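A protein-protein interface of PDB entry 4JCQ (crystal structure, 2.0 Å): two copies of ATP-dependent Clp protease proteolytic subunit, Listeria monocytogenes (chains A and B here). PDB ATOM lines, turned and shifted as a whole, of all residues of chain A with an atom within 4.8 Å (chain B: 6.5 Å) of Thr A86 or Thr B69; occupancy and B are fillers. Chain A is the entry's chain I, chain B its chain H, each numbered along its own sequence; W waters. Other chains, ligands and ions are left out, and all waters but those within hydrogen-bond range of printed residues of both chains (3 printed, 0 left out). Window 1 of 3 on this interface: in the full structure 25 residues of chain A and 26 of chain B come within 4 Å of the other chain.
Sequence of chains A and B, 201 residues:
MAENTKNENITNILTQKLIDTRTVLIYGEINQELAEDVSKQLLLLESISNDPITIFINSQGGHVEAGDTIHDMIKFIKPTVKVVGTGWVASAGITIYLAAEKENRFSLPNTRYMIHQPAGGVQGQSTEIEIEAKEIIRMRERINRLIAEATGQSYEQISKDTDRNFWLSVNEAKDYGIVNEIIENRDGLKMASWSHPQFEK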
ATOM      1  N   TYR A  27       8.358 -21.500   5.252  1.00  0.00           N
ATOM      2  CA  TYR A  27       8.410 -21.878   3.843  1.00  0.00           C
ATOM      3  C   TYR A  27       8.264 -23.392   3.715  1.00  0.00           C
ATOM      4  O   TYR A  27       8.964 -24.146   4.395  1.00  0.00           O
ATOM      5  CB  TYR A  27       9.744 -21.454   3.212  1.00  0.00           C
ATOM      6  CG  TYR A  27       9.967 -19.964   2.975  1.00  0.00           C
ATOM      7  CD1 TYR A  27      10.876 -19.535   2.010  1.00  0.00           C
ATOM      8  CD2 TYR A  27       9.289 -18.989   3.712  1.00  0.00           C
ATOM      9  CE1 TYR A  27      11.106 -18.184   1.785  1.00  0.00           C
ATOM     10  CE2 TYR A  27       9.508 -17.636   3.492  1.00  0.00           C
ATOM     11  CZ  TYR A  27      10.420 -17.239   2.528  1.00  0.00           C
ATOM     12  OH  TYR A  27      10.647 -15.899   2.308  1.00  0.00           O
ATOM     13  N   PHE A  56       7.280 -14.303   7.420  1.00  0.00           N
ATOM     14  CA  PHE A  56       7.076 -14.469   5.981  1.00  0.00           C
ATOM     15  C   PHE A  56       6.586 -15.889   5.717  1.00  0.00           C
ATOM     16  O   PHE A  56       7.238 -16.858   6.114  1.00  0.00           O
ATOM     17  CB  PHE A  56       8.368 -14.197   5.199  1.00  0.00           C
ATOM     18  CG  PHE A  56       8.801 -12.753   5.211  1.00  0.00           C
ATOM     19  CD1 PHE A  56       9.586 -12.254   6.246  1.00  0.00           C
ATOM     20  CD2 PHE A  56       8.435 -11.894   4.177  1.00  0.00           C
ATOM     21  CE1 PHE A  56       9.989 -10.925   6.256  1.00  0.00           C
ATOM     22  CE2 PHE A  56       8.836 -10.565   4.181  1.00  0.00           C
ATOM     23  CZ  PHE A  56       9.614 -10.079   5.223  1.00  0.00           C
ATOM     24  N   ILE A  57       5.433 -16.005   5.062  1.00  0.00           N
ATOM     25  CA  ILE A  57       4.812 -17.308   4.817  1.00  0.00           C
ATOM     26  C   ILE A  57       4.711 -17.622   3.325  1.00  0.00           C
ATOM     27  O   ILE A  57       4.066 -16.892   2.565  1.00  0.00           O
ATOM     28  CB  ILE A  57       3.404 -17.415   5.454  1.00  0.00           C
ATOM     29  CG1 ILE A  57       3.455 -17.080   6.949  1.00  0.00           C
ATOM     30  CG2 ILE A  57       2.828 -18.812   5.242  1.00  0.00           C
ATOM     31  CD1 ILE A  57       2.111 -16.725   7.556  1.00  0.00           C
ATOM     32  N   ASN A  58       5.368 -18.710   2.931  1.00  0.00           N
ATOM     33  CA  ASN A  58       5.237 -19.300   1.606  1.00  0.00           C
ATOM     34  C   ASN A  58       4.927 -20.784   1.792  1.00  0.00           C
ATOM     35  O   ASN A  58       5.837 -21.598   1.953  1.00  0.00           O
ATOM     36  CB  ASN A  58       6.533 -19.111   0.797  1.00  0.00           C
ATOM     37  CG  ASN A  58       6.436 -19.651  -0.626  1.00  0.00           C
ATOM     38  OD1 ASN A  58       5.712 -20.607  -0.900  1.00  0.00           O
ATOM     39  ND2 ASN A  58       7.184 -19.044  -1.537  1.00  0.00           N
ATOM     40  N   VAL A  84       3.538 -11.666   6.468  1.00  0.00           N
ATOM     41  CA  VAL A  84       3.718 -11.259   5.079  1.00  0.00           C
ATOM     42  C   VAL A  84       3.620 -12.495   4.188  1.00  0.00           C
ATOM     43  O   VAL A  84       4.499 -13.360   4.212  1.00  0.00           O
ATOM     44  CB  VAL A  84       5.078 -10.559   4.847  1.00  0.00           C
ATOM     45  CG1 VAL A  84       5.200 -10.098   3.400  1.00  0.00           C
ATOM     46  CG2 VAL A  84       5.258  -9.377   5.790  1.00  0.00           C
ATOM     47  N   GLY A  85       2.538 -12.574   3.416  1.00  0.00           N
ATOM     48  CA  GLY A  85       2.351 -13.661   2.465  1.00  0.00           C
ATOM     49  C   GLY A  85       3.240 -13.458   1.257  1.00  0.00           C
ATOM     50  O   GLY A  85       3.392 -12.332   0.771  1.00  0.00           O
ATOM     51  N   THR A  86       3.835 -14.547   0.776  1.00  0.00           N
ATOM     52  CA  THR A  86       4.721 -14.493  -0.385  1.00  0.00           C
ATOM     53  C   THR A  86       4.710 -15.806  -1.171  1.00  0.00           C
ATOM     54  O   THR A  86       4.775 -16.885  -0.586  1.00  0.00           O
ATOM     55  CB  THR A  86       6.164 -14.076   0.008  1.00  0.00           C
ATOM     56  OG1 THR A  86       7.012 -14.132  -1.142  1.00  0.00           O
ATOM     57  CG2 THR A  86       6.739 -14.971   1.114  1.00  0.00           C
ATOM     58  N   GLY A  87       4.616 -15.704  -2.497  1.00  0.00           N
ATOM     59  CA  GLY A  87       4.571 -16.883  -3.364  1.00  0.00           C
ATOM     60  C   GLY A  87       3.186 -17.497  -3.381  1.00  0.00           C
ATOM     61  O   GLY A  87       2.376 -17.192  -4.254  1.00  0.00           O
ATOM     62  N   TRP A  88       2.917 -18.377  -2.421  1.00  0.00           N
ATOM     63  CA  TRP A  88       1.549 -18.838  -2.178  1.00  0.00           C
ATOM     64  C   TRP A  88       1.256 -19.088  -0.724  1.00  0.00           C
ATOM     65  O   TRP A  88       2.158 -19.373   0.064  1.00  0.00           O
ATOM     66  CB  TRP A  88       1.157 -20.040  -3.054  1.00  0.00           C
ATOM     67  CG  TRP A  88       1.997 -21.295  -2.927  1.00  0.00           C
ATOM     68  CD1 TRP A  88       2.981 -21.587  -1.981  1.00  0.00           C
ATOM     69  CD2 TRP A  88       1.913 -22.502  -3.766  1.00  0.00           C
ATOM     70  NE1 TRP A  88       3.506 -22.838  -2.189  1.00  0.00           N
ATOM     71  CE2 TRP A  88       2.908 -23.442  -3.238  1.00  0.00           C
ATOM     72  CE3 TRP A  88       1.145 -22.877  -4.865  1.00  0.00           C
ATOM     73  CZ2 TRP A  88       3.110 -24.695  -3.804  1.00  0.00           C
ATOM     74  CZ3 TRP A  88       1.357 -24.144  -5.425  1.00  0.00           C
ATOM     75  CH2 TRP A  88       2.316 -25.028  -4.907  1.00  0.00           C
ATOM     76  N   VAL A  89      -0.015 -18.949  -0.362  1.00  0.00           N
ATOM     77  CA  VAL A  89      -0.494 -19.220   0.989  1.00  0.00           C
ATOM     78  C   VAL A  89      -1.802 -19.990   0.845  1.00  0.00           C
ATOM     79  O   VAL A  89      -2.806 -19.443   0.379  1.00  0.00           O
ATOM     80  CB  VAL A  89      -0.740 -17.923   1.798  1.00  0.00           C
ATOM     81  CG1 VAL A  89      -1.194 -18.248   3.216  1.00  0.00           C
ATOM     82  CG2 VAL A  89       0.505 -17.041   1.831  1.00  0.00           C
ATOM     83  N   LEU A 108       3.224  -9.581  -0.223  1.00  0.00           N
ATOM     84  CA  LEU A 108       4.057  -9.200  -1.352  1.00  0.00           C
ATOM     85  C   LEU A 108       3.223  -9.376  -2.630  1.00  0.00           C
ATOM     86  O   LEU A 108       2.287 -10.180  -2.641  1.00  0.00           O
ATOM     87  CB  LEU A 108       5.339 -10.042  -1.368  1.00  0.00           C
ATOM     88  CG  LEU A 108       6.613  -9.480  -0.704  1.00  0.00           C
ATOM     89  CD1 LEU A 108       6.362  -8.412   0.358  1.00  0.00           C
ATOM     90  CD2 LEU A 108       7.485 -10.596  -0.145  1.00  0.00           C
ATOM     91  N   ASN A 110       3.508 -10.698  -5.739  1.00  0.00           N
ATOM     92  CA  ASN A 110       3.422 -11.959  -6.474  1.00  0.00           C
ATOM     93  C   ASN A 110       3.081 -13.142  -5.571  1.00  0.00           C
ATOM     94  O   ASN A 110       3.918 -14.006  -5.295  1.00  0.00           O
ATOM     95  CB  ASN A 110       4.698 -12.196  -7.284  1.00  0.00           C
ATOM     96  CG  ASN A 110       4.824 -11.234  -8.449  1.00  0.00           C
ATOM     97  OD1 ASN A 110       4.137 -11.375  -9.460  1.00  0.00           O
ATOM     98  ND2 ASN A 110       5.701 -10.246  -8.312  1.00  0.00           N
ATOM     99  N   THR A 111       1.832 -13.154  -5.117  1.00  0.00           N
ATOM    100  CA  THR A 111       1.333 -14.159  -4.188  1.00  0.00           C
ATOM    101  C   THR A 111      -0.102 -14.519  -4.555  1.00  0.00           C
ATOM    102  O   THR A 111      -0.895 -13.647  -4.912  1.00  0.00           O
ATOM    103  CB  THR A 111       1.356 -13.633  -2.735  1.00  0.00           C
ATOM    104  OG1 THR A 111       2.611 -12.992  -2.472  1.00  0.00           O
ATOM    105  CG2 THR A 111       1.146 -14.768  -1.731  1.00  0.00           C
ATOM    106  N   ALA B  35      14.720 -20.572  -1.753  1.00  0.00           N
ATOM    107  CA  ALA B  35      14.019 -19.325  -1.440  1.00  0.00           C
ATOM    108  C   ALA B  35      14.214 -18.912   0.023  1.00  0.00           C
ATOM    109  O   ALA B  35      14.413 -17.731   0.310  1.00  0.00           O
ATOM    110  CB  ALA B  35      12.538 -19.436  -1.778  1.00  0.00           C
ATOM    111  N   GLU B  36      14.165 -19.885   0.932  1.00  0.00           N
ATOM    112  CA  GLU B  36      14.388 -19.632   2.356  1.00  0.00           C
ATOM    113  C   GLU B  36      15.823 -19.181   2.630  1.00  0.00           C
ATOM    114  O   GLU B  36      16.044 -18.204   3.347  1.00  0.00           O
ATOM    115  CB  GLU B  36      14.040 -20.863   3.201  1.00  0.00           C
ATOM    116  CG  GLU B  36      14.154 -20.625   4.702  1.00  0.00           C
ATOM    117  CD  GLU B  36      13.629 -21.771   5.547  1.00  0.00           C
ATOM    118  OE1 GLU B  36      12.868 -22.615   5.029  1.00  0.00           O
ATOM    119  OE2 GLU B  36      13.977 -21.821   6.745  1.00  0.00           O
ATOM    120  N   SER B  39      16.273 -15.686   1.099  1.00  0.00           N
ATOM    121  CA  SER B  39      15.543 -14.733   1.941  1.00  0.00           C
ATOM    122  C   SER B  39      16.322 -14.390   3.213  1.00  0.00           C
ATOM    123  O   SER B  39      16.434 -13.217   3.574  1.00  0.00           O
ATOM    124  CB  SER B  39      14.152 -15.262   2.302  1.00  0.00           C
ATOM    125  OG  SER B  39      13.317 -15.340   1.158  1.00  0.00           O
ATOM    126  N   VAL B  64       7.563 -21.879  -9.550  1.00  0.00           N
ATOM    127  CA  VAL B  64       7.100 -20.499  -9.747  1.00  0.00           C
ATOM    128  C   VAL B  64       6.963 -19.703  -8.440  1.00  0.00           C
ATOM    129  O   VAL B  64       7.408 -18.556  -8.362  1.00  0.00           O
ATOM    130  CB  VAL B  64       5.797 -20.439 -10.597  1.00  0.00           C
ATOM    131  CG1 VAL B  64       4.680 -21.274  -9.975  1.00  0.00           C
ATOM    132  CG2 VAL B  64       5.345 -18.999 -10.821  1.00  0.00           C
ATOM    133  N   GLU B  65       6.374 -20.322  -7.417  1.00  0.00           N
ATOM    134  CA  GLU B  65       6.111 -19.646  -6.144  1.00  0.00           C
ATOM    135  C   GLU B  65       7.397 -19.288  -5.391  1.00  0.00           C
ATOM    136  O   GLU B  65       7.456 -18.271  -4.694  1.00  0.00           O
ATOM    137  CB  GLU B  65       5.161 -20.474  -5.261  1.00  0.00           C
ATOM    138  CG  GLU B  65       5.753 -21.741  -4.649  1.00  0.00           C
ATOM    139  CD  GLU B  65       5.831 -22.921  -5.609  1.00  0.00           C
ATOM    140  OE1 GLU B  65       5.331 -22.828  -6.753  1.00  0.00           O
ATOM    141  OE2 GLU B  65       6.399 -23.959  -5.210  1.00  0.00           O
ATOM    142  N   ALA B  66       8.420 -20.127  -5.544  1.00  0.00           N
ATOM    143  CA  ALA B  66       9.736 -19.860  -4.974  1.00  0.00           C
ATOM    144  C   ALA B  66      10.422 -18.714  -5.713  1.00  0.00           C
ATOM    145  O   ALA B  66      11.077 -17.875  -5.094  1.00  0.00           O
ATOM    146  CB  ALA B  66      10.594 -21.113  -5.019  1.00  0.00           C
ATOM    147  N   GLY B  67      10.269 -18.690  -7.037  1.00  0.00           N
ATOM    148  CA  GLY B  67      10.784 -17.601  -7.864  1.00  0.00           C
ATOM    149  C   GLY B  67      10.116 -16.276  -7.539  1.00  0.00           C
ATOM    150  O   GLY B  67      10.778 -15.236  -7.498  1.00  0.00           O
ATOM    151  N   ASP B  68       8.804 -16.324  -7.304  1.00  0.00           N
ATOM    152  CA  ASP B  68       8.023 -15.144  -6.925  1.00  0.00           C
ATOM    153  C   ASP B  68       8.502 -14.537  -5.608  1.00  0.00           C
ATOM    154  O   ASP B  68       8.623 -13.315  -5.489  1.00  0.00           O
ATOM    155  CB  ASP B  68       6.532 -15.493  -6.836  1.00  0.00           C
ATOM    156  CG  ASP B  68       5.890 -15.698  -8.200  1.00  0.00           C
ATOM    157  OD1 ASP B  68       4.869 -16.415  -8.275  1.00  0.00           O
ATOM    158  OD2 ASP B  68       6.398 -15.143  -9.201  1.00  0.00           O
ATOM    159  N   THR B  69       8.775 -15.396  -4.627  1.00  0.00           N
ATOM    160  CA  THR B  69       9.274 -14.962  -3.322  1.00  0.00           C
ATOM    161  C   THR B  69      10.631 -14.266  -3.435  1.00  0.00           C
ATOM    162  O   THR B  69      10.813 -13.173  -2.898  1.00  0.00           O
ATOM    163  CB  THR B  69       9.331 -16.133  -2.312  1.00  0.00           C
ATOM    164  OG1 THR B  69       7.998 -16.521  -1.965  1.00  0.00           O
ATOM    165  CG2 THR B  69      10.061 -15.730  -1.033  1.00  0.00           C
ATOM    166  N   ILE B  70      11.570 -14.890  -4.146  1.00  0.00           N
ATOM    167  CA  ILE B  70      12.907 -14.313  -4.322  1.00  0.00           C
ATOM    168  C   ILE B  70      12.838 -12.985  -5.086  1.00  0.00           C
ATOM    169  O   ILE B  70      13.471 -12.005  -4.686  1.00  0.00           O
ATOM    170  CB  ILE B  70      13.885 -15.298  -5.002  1.00  0.00           C
ATOM    171  CG1 ILE B  70      14.061 -16.551  -4.135  1.00  0.00           C
ATOM    172  CG2 ILE B  70      15.236 -14.636  -5.243  1.00  0.00           C
ATOM    173  CD1 ILE B  70      14.675 -17.733  -4.857  1.00  0.00           C
ATOM    174  N   HIS B  71      12.060 -12.961  -6.167  1.00  0.00           N
ATOM    175  CA  HIS B  71      11.807 -11.732  -6.931  1.00  0.00           C
ATOM    176  C   HIS B  71      11.328 -10.618  -6.037  1.00  0.00           C
ATOM    177  O   HIS B  71      11.892  -9.519  -6.049  1.00  0.00           O
ATOM    178  CB  HIS B  71      10.794 -11.998  -8.046  1.00  0.00           C
ATOM    179  CG  HIS B  71      10.305 -10.747  -8.749  1.00  0.00           C
ATOM    180  ND1 HIS B  71       9.353  -9.948  -8.230  1.00  0.00           N
ATOM    181  CD2 HIS B  71      10.663 -10.185  -9.973  1.00  0.00           C
ATOM    182  CE1 HIS B  71       9.120  -8.922  -9.070  1.00  0.00           C
ATOM    183  NE2 HIS B  71       9.921  -9.068 -10.138  1.00  0.00           N
ATOM    184  N   ASP B  72      10.289 -10.897  -5.252  1.00  0.00           N
ATOM    185  CA  ASP B  72       9.673  -9.891  -4.386  1.00  0.00           C
ATOM    186  C   ASP B  72      10.562  -9.478  -3.214  1.00  0.00           C
ATOM    187  O   ASP B  72      10.551  -8.315  -2.812  1.00  0.00           O
ATOM    188  CB  ASP B  72       8.303 -10.365  -3.891  1.00  0.00           C
ATOM    189  CG  ASP B  72       7.225 -10.279  -4.963  1.00  0.00           C
ATOM    190  OD1 ASP B  72       6.066 -10.636  -4.666  1.00  0.00           O
ATOM    191  OD2 ASP B  72       7.528  -9.859  -6.101  1.00  0.00           O
ATOM    192  N   MET B  73      11.336 -10.420  -2.678  1.00  0.00           N
ATOM    193  CA  MET B  73      12.272 -10.117  -1.588  1.00  0.00           C
ATOM    194  C   MET B  73      13.389  -9.179  -2.040  1.00  0.00           C
ATOM    195  O   MET B  73      13.820  -8.308  -1.279  1.00  0.00           O
ATOM    196  CB  MET B  73      12.862 -11.397  -0.980  1.00  0.00           C
ATOM    197  CG  MET B  73      11.911 -12.172  -0.072  1.00  0.00           C
ATOM    198  SD  MET B  73      11.255 -11.254   1.343  1.00  0.00           S
ATOM    199  CE  MET B  73      12.753 -10.685   2.137  1.00  0.00           C
ATOM    200  N   ILE B  74      13.847  -9.364  -3.279  1.00  0.00           N
ATOM    201  CA  ILE B  74      14.838  -8.480  -3.896  1.00  0.00           C
ATOM    202  C   ILE B  74      14.323  -7.039  -3.955  1.00  0.00           C
ATOM    203  O   ILE B  74      15.044  -6.105  -3.605  1.00  0.00           O
ATOM    204  CB  ILE B  74      15.255  -8.982  -5.301  1.00  0.00           C
ATOM    205  CG1 ILE B  74      16.189 -10.194  -5.180  1.00  0.00           C
ATOM    206  CG2 ILE B  74      15.934  -7.880  -6.108  1.00  0.00           C
ATOM    207  CD1 ILE B  74      16.340 -10.996  -6.457  1.00  0.00           C
HETATM  208  O   HOH W   1      10.659 -22.462   6.881  1.00  0.00           O
HETATM  209  O   HOH W   2       5.861 -13.081  -3.267  1.00  0.00           O
HETATM  210  O   HOH W   3       2.613 -16.980  -6.962  1.00  0.00           O
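The side-chain hydroxyl (OG) of Ser B39 lies within hydrogen-bond range of the side-chain hydroxyl (OH) of Tyr A27, 3.0 Å away. The side-chain amide nitrogen (ND2) of Asn A58 is in hydrogen-bond range of the backbone carbonyl oxygen (O) of Glu B65 (3.3 Å). The side-chain hydroxyl (OG1) of Thr B69 is in hydrogen-bond range of the side-chain amide nitrogen (ND2) of Asn A58 (2.7 Å). The side-chain hydroxyl of Thr B69 sits at hydrogen-bond distance from the side-chain hydroxyl of Thr A86. OD1 of Asp B72 sits at hydrogen-bond distance from N of Asn A110 (2.8 Å).
The side-chain hydroxyl of Ser B39 is in hydrogen-bond range of the backbone carbonyl oxygen of Ala B35, at 2.8 Å. A ring nitrogen (ND1) of His B71 lies within hydrogen-bond range of the side-chain carboxylate (OD2) of Asp B72, at 2.8 Å. The backbone NH (N) of Thr A86 lies within hydrogen-bond range of the backbone carbonyl oxygen (O) of Ile A57 (3.0 Å). The side-chain amide nitrogen (ND2) of Asn A58 sits close to the backbone carbonyl oxygen (O) of Thr A86, at 3.4 Å. N of Gly A87 lies within hydrogen-bond range of O of Asn A110, at 3.3 Å. OG1 of Thr A111 sits at hydrogen-bond distance from N of Gly A87, at 3.4 Å.
Among the printed residues, pairs that only touch across the chains: Tyr A27 with Ala B35 (3.6 Å), Tyr A27 with Glu B36 (3.5 Å), Tyr A27 with Thr B69 (3.4 Å), Phe A56 with Met B73 (3.8 Å), Gly A87 with Glu B65 (3.5 Å), Gly A87 with Thr B69 (3.5 Å), Trp A88 with Glu B65 (3.5 Å), Leu A108 with Asp B72 (3.4 Å), Asn A110 with Asp B68 (3.4 Å) and Asn A110 with His B71 (3.7 Å).
Of chain B, only Thr B69 comes within 4 Å of Thr A86. Thr B69 touches just these residues of chain A: Tyr A27, Asn A58, Thr A86 and Gly A87. Printed residues of chain A within 4 Å of Asp B68: Asn A110 (3.4 Å). Printed residues of chain A within 4 Å of His B71: Asn A110 (3.7 Å). Of the printed residues of chain B, Tyr A27 touches Ala B35, Glu B36, Ser B39 and Thr B69. Of the printed residues of chain A, Glu B36 touches Tyr A27. Of the printed residues of chain A, Glu B65 touches Asn A58, Gly A87 and Trp A88. The nearest residue of chain B that does not touch Thr A86 is Asp B68 (4.7 Å).
Hydrophobic or aromatic side chains of chain A within 4 Å of the printed part of chain B: Tyr A27, Phe A56, Trp A88 and Leu A108. Along chain A the printed residues that touch a printed residue of chain B span positions 27 to 110. Among the printed residues, 15 pairs touch across the chains. Among the printed residues, no Asp or Glu carboxylate lies within 4 Å of a Lys or Arg side-chain nitrogen of the other chain.
No position is printed for both chains.
Water W2 lies within hydrogen-bond range of the side-chain hydroxyl of Thr A86 (2.6 Å), the side-chain carboxylate of Asp B72 (2.8 Å), the backbone carbonyl oxygen of Asn A110 (3.0 Å), the backbone NH of Gly A87 (3.0 Å) and the side-chain hydroxyl of Thr A111 (3.3 Å). Water W3 bridges OD1 of Asp B68 and O of Gly A87. Water W1 bridges the side-chain carboxylate (OE1) of Glu B36 (2.9 Å) and the backbone NH (N) of Tyr A27 (3.0 Å).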
